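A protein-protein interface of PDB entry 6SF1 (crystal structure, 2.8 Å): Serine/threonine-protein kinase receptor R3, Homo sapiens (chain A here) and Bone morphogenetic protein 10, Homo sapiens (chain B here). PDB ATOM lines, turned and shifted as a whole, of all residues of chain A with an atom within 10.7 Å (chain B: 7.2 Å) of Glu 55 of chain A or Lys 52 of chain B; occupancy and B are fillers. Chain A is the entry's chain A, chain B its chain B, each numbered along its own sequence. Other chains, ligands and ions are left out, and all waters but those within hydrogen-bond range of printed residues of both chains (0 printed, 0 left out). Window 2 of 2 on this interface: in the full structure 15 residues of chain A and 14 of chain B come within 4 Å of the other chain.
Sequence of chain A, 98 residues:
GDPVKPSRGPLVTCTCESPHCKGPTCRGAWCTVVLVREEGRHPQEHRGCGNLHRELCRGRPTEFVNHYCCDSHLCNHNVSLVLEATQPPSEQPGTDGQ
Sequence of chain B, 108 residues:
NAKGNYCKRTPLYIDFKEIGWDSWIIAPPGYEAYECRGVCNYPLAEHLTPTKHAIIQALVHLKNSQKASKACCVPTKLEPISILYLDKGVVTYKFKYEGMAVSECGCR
The side-chain sulfur (SG) of Cys 57 of chain A is disulfide-bonded to the side-chain sulfur (SG) of Cys 69 of chain A (2.0 Å).
Among the printed residues, pairs that only touch across the chains: His 53 of chain A with Pro 50 of chain B (3.1 Å), His 53 of chain A with Lys 52 of chain B (3.5 Å), His 53 of chain A with Ile 55 of chain B (3.4 Å), Glu 55 of chain A with Lys 52 of chain B (3.3 Å) and Leu 56 of chain A with Ile 55 of chain B (3.7 Å).
Leu 52 of chain A touches none of the printed residues of chain B. Of the printed residues of chain B, His 53 of chain A touches Pro 50, Lys 52 and Ile 55. Arg 54 of chain A touches none of the printed residues of chain B. Glu 55 of chain A touches just one residue of chain B: Lys 52 (3.3 Å). Printed residues of chain B within 4 Å of Leu 56 of chain A: Ile 55 (3.7 Å). Of the printed residues of chain A, Pro 50 of chain B touches His 53 (3.1 Å). No residue of chain A comes within 4 Å of Thr 51 of chain B. Of chain A, only His 53 and Glu 55 come within 4 Å of Lys 52 of chain B. No residue of chain A comes within 4 Å of Ala 54 of chain B. Ile 55 of chain B touches just these residues of chain A: His 53 (3.4 Å) and Leu 56 (3.7 Å). No residue of chain A comes within 4 Å of Ile 56 of chain B. The nearest printed residue of chain A that does not touch Pro 50 of chain B is Leu 52 of chain A (5.9 Å).
Hydrophobic or aromatic side chains of chain A within 4 Å of the printed part of chain B: His 53 and Leu 56. Along chain A the printed residues that touch a printed residue of chain B span positions 53 to 56. Hydrophobic or aromatic side chains of chain B within 4 Å of the printed part of chain A: Ile 55. Among the printed residues, 5 pairs touch across the chains. Among the printed residues, no Asp or Glu carboxylate lies within 4 Å of a Lys or Arg side-chain nitrogen of the other chain.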
ATOM      1  N   TRP A  30     -31.962  -6.941  -6.801  1.00  0.00           N
ATOM      2  CA  TRP A  30     -30.906  -6.007  -6.440  1.00  0.00           C
ATOM      3  C   TRP A  30     -31.326  -4.605  -6.852  1.00  0.00           C
ATOM      4  O   TRP A  30     -32.162  -4.422  -7.741  1.00  0.00           O
ATOM      5  CB  TRP A  30     -29.568  -6.380  -7.094  1.00  0.00           C
ATOM      6  CG  TRP A  30     -29.597  -6.334  -8.590  1.00  0.00           C
ATOM      7  CD1 TRP A  30     -29.402  -5.239  -9.379  1.00  0.00           C
ATOM      8  CD2 TRP A  30     -29.832  -7.432  -9.478  1.00  0.00           C
ATOM      9  NE1 TRP A  30     -29.507  -5.586 -10.705  1.00  0.00           N
ATOM     10  CE2 TRP A  30     -29.770  -6.927 -10.791  1.00  0.00           C
ATOM     11  CE3 TRP A  30     -30.092  -8.793  -9.290  1.00  0.00           C
ATOM     12  CZ2 TRP A  30     -29.958  -7.733 -11.911  1.00  0.00           C
ATOM     13  CZ3 TRP A  30     -30.279  -9.592 -10.403  1.00  0.00           C
ATOM     14  CH2 TRP A  30     -30.212  -9.059 -11.697  1.00  0.00           C
ATOM     15  N   THR A  32     -30.479  -0.842  -8.417  1.00  0.00           N
ATOM     16  CA  THR A  32     -29.677  -0.365  -9.535  1.00  0.00           C
ATOM     17  C   THR A  32     -29.616   1.155  -9.552  1.00  0.00           C
ATOM     18  O   THR A  32     -30.599   1.833  -9.235  1.00  0.00           O
ATOM     19  CB  THR A  32     -30.235  -0.853 -10.878  1.00  0.00           C
ATOM     20  OG1 THR A  32     -31.526  -0.273 -11.101  1.00  0.00           O
ATOM     21  CG2 THR A  32     -30.357  -2.364 -10.893  1.00  0.00           C
ATOM     22  N   VAL A  34     -28.215   3.551 -12.703  1.00  0.00           N
ATOM     23  CA  VAL A  34     -27.675   3.531 -14.057  1.00  0.00           C
ATOM     24  C   VAL A  34     -27.518   4.969 -14.527  1.00  0.00           C
ATOM     25  O   VAL A  34     -28.508   5.704 -14.637  1.00  0.00           O
ATOM     26  CB  VAL A  34     -28.568   2.734 -15.019  1.00  0.00           C
ATOM     27  CG1 VAL A  34     -27.839   2.482 -16.330  1.00  0.00           C
ATOM     28  CG2 VAL A  34     -29.000   1.421 -14.382  1.00  0.00           C
ATOM     29  N   GLY A  50     -33.384  -4.415 -10.025  1.00  0.00           N
ATOM     30  CA  GLY A  50     -32.942  -5.292 -11.088  1.00  0.00           C
ATOM     31  C   GLY A  50     -33.191  -6.753 -10.772  1.00  0.00           C
ATOM     32  O   GLY A  50     -32.832  -7.231  -9.693  1.00  0.00           O
ATOM     33  N   ASN A  51     -33.822  -7.467 -11.702  1.00  0.00           N
ATOM     34  CA  ASN A  51     -34.061  -8.894 -11.558  1.00  0.00           C
ATOM     35  C   ASN A  51     -33.430  -9.731 -12.657  1.00  0.00           C
ATOM     36  O   ASN A  51     -33.162 -10.915 -12.427  1.00  0.00           O
ATOM     37  CB  ASN A  51     -35.570  -9.190 -11.524  1.00  0.00           C
ATOM     38  CG  ASN A  51     -36.273  -8.506 -10.370  1.00  0.00           C
ATOM     39  OD1 ASN A  51     -36.377  -9.061  -9.275  1.00  0.00           O
ATOM     40  ND2 ASN A  51     -36.763  -7.294 -10.607  1.00  0.00           N
ATOM     41  N   LEU A  52     -33.184  -9.158 -13.831  1.00  0.00           N
ATOM     42  CA  LEU A  52     -32.601  -9.871 -14.953  1.00  0.00           C
ATOM     43  C   LEU A  52     -31.315  -9.182 -15.388  1.00  0.00           C
ATOM     44  O   LEU A  52     -31.096  -7.997 -15.113  1.00  0.00           O
ATOM     45  CB  LEU A  52     -33.580  -9.944 -16.133  1.00  0.00           C
ATOM     46  CG  LEU A  52     -35.007 -10.379 -15.796  1.00  0.00           C
ATOM     47  CD1 LEU A  52     -35.878 -10.360 -17.041  1.00  0.00           C
ATOM     48  CD2 LEU A  52     -35.018 -11.755 -15.147  1.00  0.00           C
ATOM     49  N   HIS A  53     -30.467  -9.945 -16.072  1.00  0.00           N
ATOM     50  CA  HIS A  53     -29.206  -9.450 -16.621  1.00  0.00           C
ATOM     51  C   HIS A  53     -28.350  -8.803 -15.531  1.00  0.00           C
ATOM     52  O   HIS A  53     -28.030  -7.613 -15.566  1.00  0.00           O
ATOM     53  CB  HIS A  53     -29.461  -8.483 -17.780  1.00  0.00           C
ATOM     54  CG  HIS A  53     -30.361  -9.038 -18.838  1.00  0.00           C
ATOM     55  ND1 HIS A  53     -31.666  -8.624 -18.997  1.00  0.00           N
ATOM     56  CD2 HIS A  53     -30.149  -9.985 -19.782  1.00  0.00           C
ATOM     57  CE1 HIS A  53     -32.216  -9.286 -19.999  1.00  0.00           C
ATOM     58  NE2 HIS A  53     -31.317 -10.118 -20.493  1.00  0.00           N
ATOM     59  N   ARG A  54     -27.991  -9.624 -14.542  1.00  0.00           N
ATOM     60  CA  ARG A  54     -27.092  -9.172 -13.486  1.00  0.00           C
ATOM     61  C   ARG A  54     -25.732  -8.781 -14.047  1.00  0.00           C
ATOM     62  O   ARG A  54     -25.039  -7.936 -13.469  1.00  0.00           O
ATOM     63  CB  ARG A  54     -26.950 -10.267 -12.427  1.00  0.00           C
ATOM     64  CG  ARG A  54     -25.925  -9.982 -11.342  1.00  0.00           C
ATOM     65  CD  ARG A  54     -26.559 -10.001  -9.964  1.00  0.00           C
ATOM     66  NE  ARG A  54     -27.282 -11.241  -9.705  1.00  0.00           N
ATOM     67  CZ  ARG A  54     -27.850 -11.542  -8.541  1.00  0.00           C
ATOM     68  NH1 ARG A  54     -27.776 -10.692  -7.526  1.00  0.00           N
ATOM     69  NH2 ARG A  54     -28.490 -12.693  -8.391  1.00  0.00           N
ATOM     70  N   GLU A  55     -25.347  -9.367 -15.184  1.00  0.00           N
ATOM     71  CA  GLU A  55     -24.053  -9.078 -15.787  1.00  0.00           C
ATOM     72  C   GLU A  55     -23.906  -7.618 -16.196  1.00  0.00           C
ATOM     73  O   GLU A  55     -22.777  -7.153 -16.389  1.00  0.00           O
ATOM     74  CB  GLU A  55     -23.830  -9.987 -16.997  1.00  0.00           C
ATOM     75  CG  GLU A  55     -24.963  -9.981 -18.015  1.00  0.00           C
ATOM     76  CD  GLU A  55     -26.063 -10.974 -17.680  1.00  0.00           C
ATOM     77  OE1 GLU A  55     -26.004 -11.590 -16.594  1.00  0.00           O
ATOM     78  OE2 GLU A  55     -26.987 -11.139 -18.504  1.00  0.00           O
ATOM     79  N   LEU A  56     -25.014  -6.885 -16.340  1.00  0.00           N
ATOM     80  CA  LEU A  56     -24.918  -5.450 -16.582  1.00  0.00           C
ATOM     81  C   LEU A  56     -24.224  -4.738 -15.430  1.00  0.00           C
ATOM     82  O   LEU A  56     -23.539  -3.732 -15.641  1.00  0.00           O
ATOM     83  CB  LEU A  56     -26.309  -4.855 -16.804  1.00  0.00           C
ATOM     84  CG  LEU A  56     -27.008  -5.207 -18.116  1.00  0.00           C
ATOM     85  CD1 LEU A  56     -28.374  -4.544 -18.193  1.00  0.00           C
ATOM     86  CD2 LEU A  56     -26.144  -4.796 -19.293  1.00  0.00           C
ATOM     87  N   CYS A  57     -24.383  -5.253 -14.208  1.00  0.00           N
ATOM     88  CA  CYS A  57     -23.760  -4.635 -13.044  1.00  0.00           C
ATOM     89  C   CYS A  57     -22.242  -4.733 -13.092  1.00  0.00           C
ATOM     90  O   CYS A  57     -21.548  -3.890 -12.511  1.00  0.00           O
ATOM     91  CB  CYS A  57     -24.287  -5.292 -11.773  1.00  0.00           C
ATOM     92  SG  CYS A  57     -26.078  -5.238 -11.612  1.00  0.00           S
ATOM     93  N   ARG A  58     -21.709  -5.748 -13.769  1.00  0.00           N
ATOM     94  CA  ARG A  58     -20.271  -5.976 -13.796  1.00  0.00           C
ATOM     95  C   ARG A  58     -19.556  -5.154 -14.859  1.00  0.00           C
ATOM     96  O   ARG A  58     -18.323  -5.180 -14.908  1.00  0.00           O
ATOM     97  CB  ARG A  58     -19.987  -7.461 -14.021  1.00  0.00           C
ATOM     98  CG  ARG A  58     -20.812  -8.382 -13.139  1.00  0.00           C
ATOM     99  CD  ARG A  58     -20.449  -9.837 -13.368  1.00  0.00           C
ATOM    100  NE  ARG A  58     -19.036 -10.086 -13.105  1.00  0.00           N
ATOM    101  CZ  ARG A  58     -18.439 -11.257 -13.298  1.00  0.00           C
ATOM    102  NH1 ARG A  58     -19.133 -12.289 -13.757  1.00  0.00           N
ATOM    103  NH2 ARG A  58     -17.148 -11.395 -13.033  1.00  0.00           N
ATOM    104  N   GLY A  59     -20.291  -4.429 -15.698  1.00  0.00           N
ATOM    105  CA  GLY A  59     -19.661  -3.686 -16.777  1.00  0.00           C
ATOM    106  C   GLY A  59     -18.831  -2.532 -16.245  1.00  0.00           C
ATOM    107  O   GLY A  59     -19.279  -1.771 -15.378  1.00  0.00           O
ATOM    108  N   ARG A  60     -17.614  -2.402 -16.760  1.00  0.00           N
ATOM    109  CA  ARG A  60     -16.763  -1.284 -16.383  1.00  0.00           C
ATOM    110  C   ARG A  60     -17.383   0.025 -16.870  1.00  0.00           C
ATOM    111  O   ARG A  60     -17.919   0.081 -17.980  1.00  0.00           O
ATOM    112  CB  ARG A  60     -15.362  -1.456 -16.972  1.00  0.00           C
ATOM    113  CG  ARG A  60     -14.412  -0.303 -16.686  1.00  0.00           C
ATOM    114  CD  ARG A  60     -13.043  -0.522 -17.315  1.00  0.00           C
ATOM    115  NE  ARG A  60     -13.112  -0.608 -18.771  1.00  0.00           N
ATOM    116  CZ  ARG A  60     -13.079  -1.746 -19.455  1.00  0.00           C
ATOM    117  NH1 ARG A  60     -12.973  -2.903 -18.815  1.00  0.00           N
ATOM    118  NH2 ARG A  60     -13.149  -1.729 -20.779  1.00  0.00           N
ATOM    119  N   PRO A  61     -17.345   1.080 -16.057  1.00  0.00           N
ATOM    120  CA  PRO A  61     -17.892   2.369 -16.503  1.00  0.00           C
ATOM    121  C   PRO A  61     -17.185   2.872 -17.754  1.00  0.00           C
ATOM    122  O   PRO A  61     -15.962   2.782 -17.880  1.00  0.00           O
ATOM    123  CB  PRO A  61     -17.642   3.292 -15.305  1.00  0.00           C
ATOM    124  CG  PRO A  61     -17.569   2.370 -14.132  1.00  0.00           C
ATOM    125  CD  PRO A  61     -16.930   1.113 -14.645  1.00  0.00           C
ATOM    126  N   VAL A  65     -21.960   5.018 -20.172  1.00  0.00           N
ATOM    127  CA  VAL A  65     -22.817   4.231 -19.289  1.00  0.00           C
ATOM    128  C   VAL A  65     -22.030   3.854 -18.042  1.00  0.00           C
ATOM    129  O   VAL A  65     -20.814   3.642 -18.093  1.00  0.00           O
ATOM    130  CB  VAL A  65     -23.376   2.985 -20.016  1.00  0.00           C
ATOM    131  CG1 VAL A  65     -22.267   1.998 -20.342  1.00  0.00           C
ATOM    132  CG2 VAL A  65     -24.468   2.325 -19.190  1.00  0.00           C
ATOM    133  N   ASN A  66     -22.734   3.799 -16.911  1.00  0.00           N
ATOM    134  CA  ASN A  66     -22.173   3.333 -15.647  1.00  0.00           C
ATOM    135  C   ASN A  66     -23.269   2.599 -14.893  1.00  0.00           C
ATOM    136  O   ASN A  66     -24.329   3.173 -14.624  1.00  0.00           O
ATOM    137  CB  ASN A  66     -21.624   4.494 -14.810  1.00  0.00           C
ATOM    138  CG  ASN A  66     -20.791   4.023 -13.625  1.00  0.00           C
ATOM    139  OD1 ASN A  66     -21.025   2.951 -13.067  1.00  0.00           O
ATOM    140  ND2 ASN A  66     -19.811   4.831 -13.238  1.00  0.00           N
ATOM    141  N   HIS A  67     -23.018   1.339 -14.556  1.00  0.00           N
ATOM    142  CA  HIS A  67     -23.976   0.500 -13.848  1.00  0.00           C
ATOM    143  C   HIS A  67     -23.506   0.289 -12.416  1.00  0.00           C
ATOM    144  O   HIS A  67     -22.429  -0.276 -12.189  1.00  0.00           O
ATOM    145  CB  HIS A  67     -24.148  -0.848 -14.545  1.00  0.00           C
ATOM    146  CG  HIS A  67     -25.079  -0.811 -15.715  1.00  0.00           C
ATOM    147  ND1 HIS A  67     -26.423  -1.098 -15.605  1.00  0.00           N
ATOM    148  CD2 HIS A  67     -24.860  -0.530 -17.022  1.00  0.00           C
ATOM    149  CE1 HIS A  67     -26.992  -0.991 -16.792  1.00  0.00           C
ATOM    150  NE2 HIS A  67     -26.065  -0.649 -17.669  1.00  0.00           N
ATOM    151  N   TYR A  68     -24.312   0.734 -11.460  1.00  0.00           N
ATOM    152  CA  TYR A  68     -24.098   0.452 -10.050  1.00  0.00           C
ATOM    153  C   TYR A  68     -25.217  -0.450  -9.550  1.00  0.00           C
ATOM    154  O   TYR A  68     -26.386  -0.251  -9.894  1.00  0.00           O
ATOM    155  CB  TYR A  68     -24.052   1.739  -9.224  1.00  0.00           C
ATOM    156  CG  TYR A  68     -23.795   1.511  -7.752  1.00  0.00           C
ATOM    157  CD1 TYR A  68     -24.848   1.374  -6.855  1.00  0.00           C
ATOM    158  CD2 TYR A  68     -22.499   1.432  -7.257  1.00  0.00           C
ATOM    159  CE1 TYR A  68     -24.618   1.164  -5.510  1.00  0.00           C
ATOM    160  CE2 TYR A  68     -22.259   1.223  -5.913  1.00  0.00           C
ATOM    161  CZ  TYR A  68     -23.323   1.090  -5.046  1.00  0.00           C
ATOM    162  OH  TYR A  68     -23.092   0.881  -3.706  1.00  0.00           O
ATOM    163  N   CYS A  69     -24.857  -1.447  -8.746  1.00  0.00           N
ATOM    164  CA  CYS A  69     -25.833  -2.391  -8.225  1.00  0.00           C
ATOM    165  C   CYS A  69     -25.501  -2.746  -6.785  1.00  0.00           C
ATOM    166  O   CYS A  69     -24.331  -2.818  -6.396  1.00  0.00           O
ATOM    167  CB  CYS A  69     -25.897  -3.669  -9.066  1.00  0.00           C
ATOM    168  SG  CYS A  69     -26.398  -3.420 -10.777  1.00  0.00           S
ATOM    169  N   LEU B  44     -32.777  -0.451 -20.802  1.00  0.00           N
ATOM    170  CA  LEU B  44     -34.017  -1.083 -21.234  1.00  0.00           C
ATOM    171  C   LEU B  44     -34.709  -1.717 -20.031  1.00  0.00           C
ATOM    172  O   LEU B  44     -34.166  -2.632 -19.405  1.00  0.00           O
ATOM    173  CB  LEU B  44     -33.731  -2.127 -22.310  1.00  0.00           C
ATOM    174  CG  LEU B  44     -32.930  -1.632 -23.518  1.00  0.00           C
ATOM    175  CD1 LEU B  44     -32.787  -2.727 -24.569  1.00  0.00           C
ATOM    176  CD2 LEU B  44     -33.566  -0.386 -24.118  1.00  0.00           C
ATOM    177  N   THR B  49     -39.091  -6.935 -21.251  1.00  0.00           N
ATOM    178  CA  THR B  49     -38.357  -8.174 -21.497  1.00  0.00           C
ATOM    179  C   THR B  49     -37.281  -8.025 -22.570  1.00  0.00           C
ATOM    180  O   THR B  49     -37.292  -8.770 -23.558  1.00  0.00           O
ATOM    181  CB  THR B  49     -39.324  -9.293 -21.895  1.00  0.00           C
ATOM    182  OG1 THR B  49     -40.135  -8.863 -22.997  1.00  0.00           O
ATOM    183  CG2 THR B  49     -40.221  -9.664 -20.723  1.00  0.00           C
ATOM    184  N   PRO B  50     -36.337  -7.096 -22.418  1.00  0.00           N
ATOM    185  CA  PRO B  50     -35.343  -6.896 -23.477  1.00  0.00           C
ATOM    186  C   PRO B  50     -34.355  -8.049 -23.529  1.00  0.00           C
ATOM    187  O   PRO B  50     -33.873  -8.528 -22.500  1.00  0.00           O
ATOM    188  CB  PRO B  50     -34.658  -5.586 -23.074  1.00  0.00           C
ATOM    189  CG  PRO B  50     -34.761  -5.569 -21.590  1.00  0.00           C
ATOM    190  CD  PRO B  50     -36.064  -6.248 -21.242  1.00  0.00           C
ATOM    191  N   THR B  51     -34.065  -8.499 -24.744  1.00  0.00           N
ATOM    192  CA  THR B  51     -33.082  -9.548 -24.939  1.00  0.00           C
ATOM    193  C   THR B  51     -31.672  -8.985 -24.771  1.00  0.00           C
ATOM    194  O   THR B  51     -31.453  -7.771 -24.761  1.00  0.00           O
ATOM    195  CB  THR B  51     -33.242 -10.184 -26.318  1.00  0.00           C
ATOM    196  OG1 THR B  51     -33.041  -9.191 -27.331  1.00  0.00           O
ATOM    197  CG2 THR B  51     -34.633 -10.778 -26.471  1.00  0.00           C
ATOM    198  N   LYS B  52     -30.702  -9.891 -24.637  1.00  0.00           N
ATOM    199  CA  LYS B  52     -29.321  -9.457 -24.449  1.00  0.00           C
ATOM    200  C   LYS B  52     -28.786  -8.737 -25.678  1.00  0.00           C
ATOM    201  O   LYS B  52     -27.992  -7.798 -25.543  1.00  0.00           O
ATOM    202  CB  LYS B  52     -28.436 -10.650 -24.091  1.00  0.00           C
ATOM    203  CG  LYS B  52     -28.727 -11.215 -22.711  1.00  0.00           C
ATOM    204  CD  LYS B  52     -27.837 -12.397 -22.380  1.00  0.00           C
ATOM    205  CE  LYS B  52     -28.171 -12.953 -21.006  1.00  0.00           C
ATOM    206  NZ  LYS B  52     -29.591 -13.390 -20.916  1.00  0.00           N
ATOM    207  N   HIS B  53     -29.206  -9.147 -26.876  1.00  0.00           N
ATOM    208  CA  HIS B  53     -28.788  -8.429 -28.076  1.00  0.00           C
ATOM    209  C   HIS B  53     -29.360  -7.017 -28.095  1.00  0.00           C
ATOM    210  O   HIS B  53     -28.670  -6.068 -28.487  1.00  0.00           O
ATOM    211  CB  HIS B  53     -29.210  -9.191 -29.330  1.00  0.00           C
ATOM    212  CG  HIS B  53     -28.866  -8.483 -30.604  1.00  0.00           C
ATOM    213  ND1 HIS B  53     -29.688  -7.537 -31.176  1.00  0.00           N
ATOM    214  CD2 HIS B  53     -27.781  -8.574 -31.409  1.00  0.00           C
ATOM    215  CE1 HIS B  53     -29.127  -7.077 -32.280  1.00  0.00           C
ATOM    216  NE2 HIS B  53     -27.969  -7.691 -32.444  1.00  0.00           N
ATOM    217  N   ALA B  54     -30.619  -6.860 -27.678  1.00  0.00           N
ATOM    218  CA  ALA B  54     -31.215  -5.530 -27.616  1.00  0.00           C
ATOM    219  C   ALA B  54     -30.476  -4.643 -26.624  1.00  0.00           C
ATOM    220  O   ALA B  54     -30.250  -3.456 -26.890  1.00  0.00           O
ATOM    221  CB  ALA B  54     -32.695  -5.633 -27.246  1.00  0.00           C
ATOM    222  N   ILE B  55     -30.086  -5.204 -25.478  1.00  0.00           N
ATOM    223  CA  ILE B  55     -29.331  -4.437 -24.492  1.00  0.00           C
ATOM    224  C   ILE B  55     -27.964  -4.056 -25.046  1.00  0.00           C
ATOM    225  O   ILE B  55     -27.498  -2.925 -24.862  1.00  0.00           O
ATOM    226  CB  ILE B  55     -29.210  -5.230 -23.180  1.00  0.00           C
ATOM    227  CG1 ILE B  55     -30.596  -5.519 -22.600  1.00  0.00           C
ATOM    228  CG2 ILE B  55     -28.360  -4.471 -22.176  1.00  0.00           C
ATOM    229  CD1 ILE B  55     -30.568  -6.386 -21.362  1.00  0.00           C
ATOM    230  N   ILE B  56     -27.303  -4.989 -25.734  1.00  0.00           N
ATOM    231  CA  ILE B  56     -25.998  -4.699 -26.320  1.00  0.00           C
ATOM    232  C   ILE B  56     -26.129  -3.661 -27.428  1.00  0.00           C
ATOM    233  O   ILE B  56     -25.346  -2.708 -27.505  1.00  0.00           O
ATOM    234  CB  ILE B  56     -25.344  -5.992 -26.837  1.00  0.00           C
ATOM    235  CG1 ILE B  56     -24.937  -6.887 -25.669  1.00  0.00           C
ATOM    236  CG2 ILE B  56     -24.142  -5.672 -27.707  1.00  0.00           C
ATOM    237  CD1 ILE B  56     -24.307  -8.184 -26.099  1.00  0.00           C
ATOM    238  N   GLN B  57     -27.123  -3.833 -28.305  1.00  0.00           N
ATOM    239  CA  GLN B  57     -27.328  -2.875 -29.386  1.00  0.00           C
ATOM    240  C   GLN B  57     -27.643  -1.486 -28.848  1.00  0.00           C
ATOM    241  O   GLN B  57     -27.235  -0.481 -29.444  1.00  0.00           O
ATOM    242  CB  GLN B  57     -28.446  -3.358 -30.309  1.00  0.00           C
ATOM    243  CG  GLN B  57     -28.734  -2.431 -31.475  1.00  0.00           C
ATOM    244  CD  GLN B  57     -29.906  -2.897 -32.313  1.00  0.00           C
ATOM    245  OE1 GLN B  57     -30.127  -4.097 -32.478  1.00  0.00           O
ATOM    246  NE2 GLN B  57     -30.671  -1.949 -32.841  1.00  0.00           N
ATOM    247  N   ALA B  58     -28.358  -1.407 -27.724  1.00  0.00           N
ATOM    248  CA  ALA B  58     -28.610  -0.114 -27.099  1.00  0.00           C
ATOM    249  C   ALA B  58     -27.330   0.501 -26.551  1.00  0.00           C
ATOM    250  O   ALA B  58     -27.204   1.730 -26.508  1.00  0.00           O
ATOM    251  CB  ALA B  58     -29.649  -0.260 -25.987  1.00  0.00           C
ATOM    252  N   LEU B  59     -26.372  -0.332 -26.135  1.00  0.00           N
ATOM    253  CA  LEU B  59     -25.119   0.191 -25.601  1.00  0.00           C
ATOM    254  C   LEU B  59     -24.233   0.752 -26.706  1.00  0.00           C
ATOM    255  O   LEU B  59     -23.545   1.760 -26.505  1.00  0.00           O
ATOM    256  CB  LEU B  59     -24.384  -0.903 -24.826  1.00  0.00           C
ATOM    257  CG  LEU B  59     -24.980  -1.261 -23.465  1.00  0.00           C
ATOM    258  CD1 LEU B  59     -24.234  -2.424 -22.834  1.00  0.00           C
ATOM    259  CD2 LEU B  59     -24.956  -0.047 -22.554  1.00  0.00           C
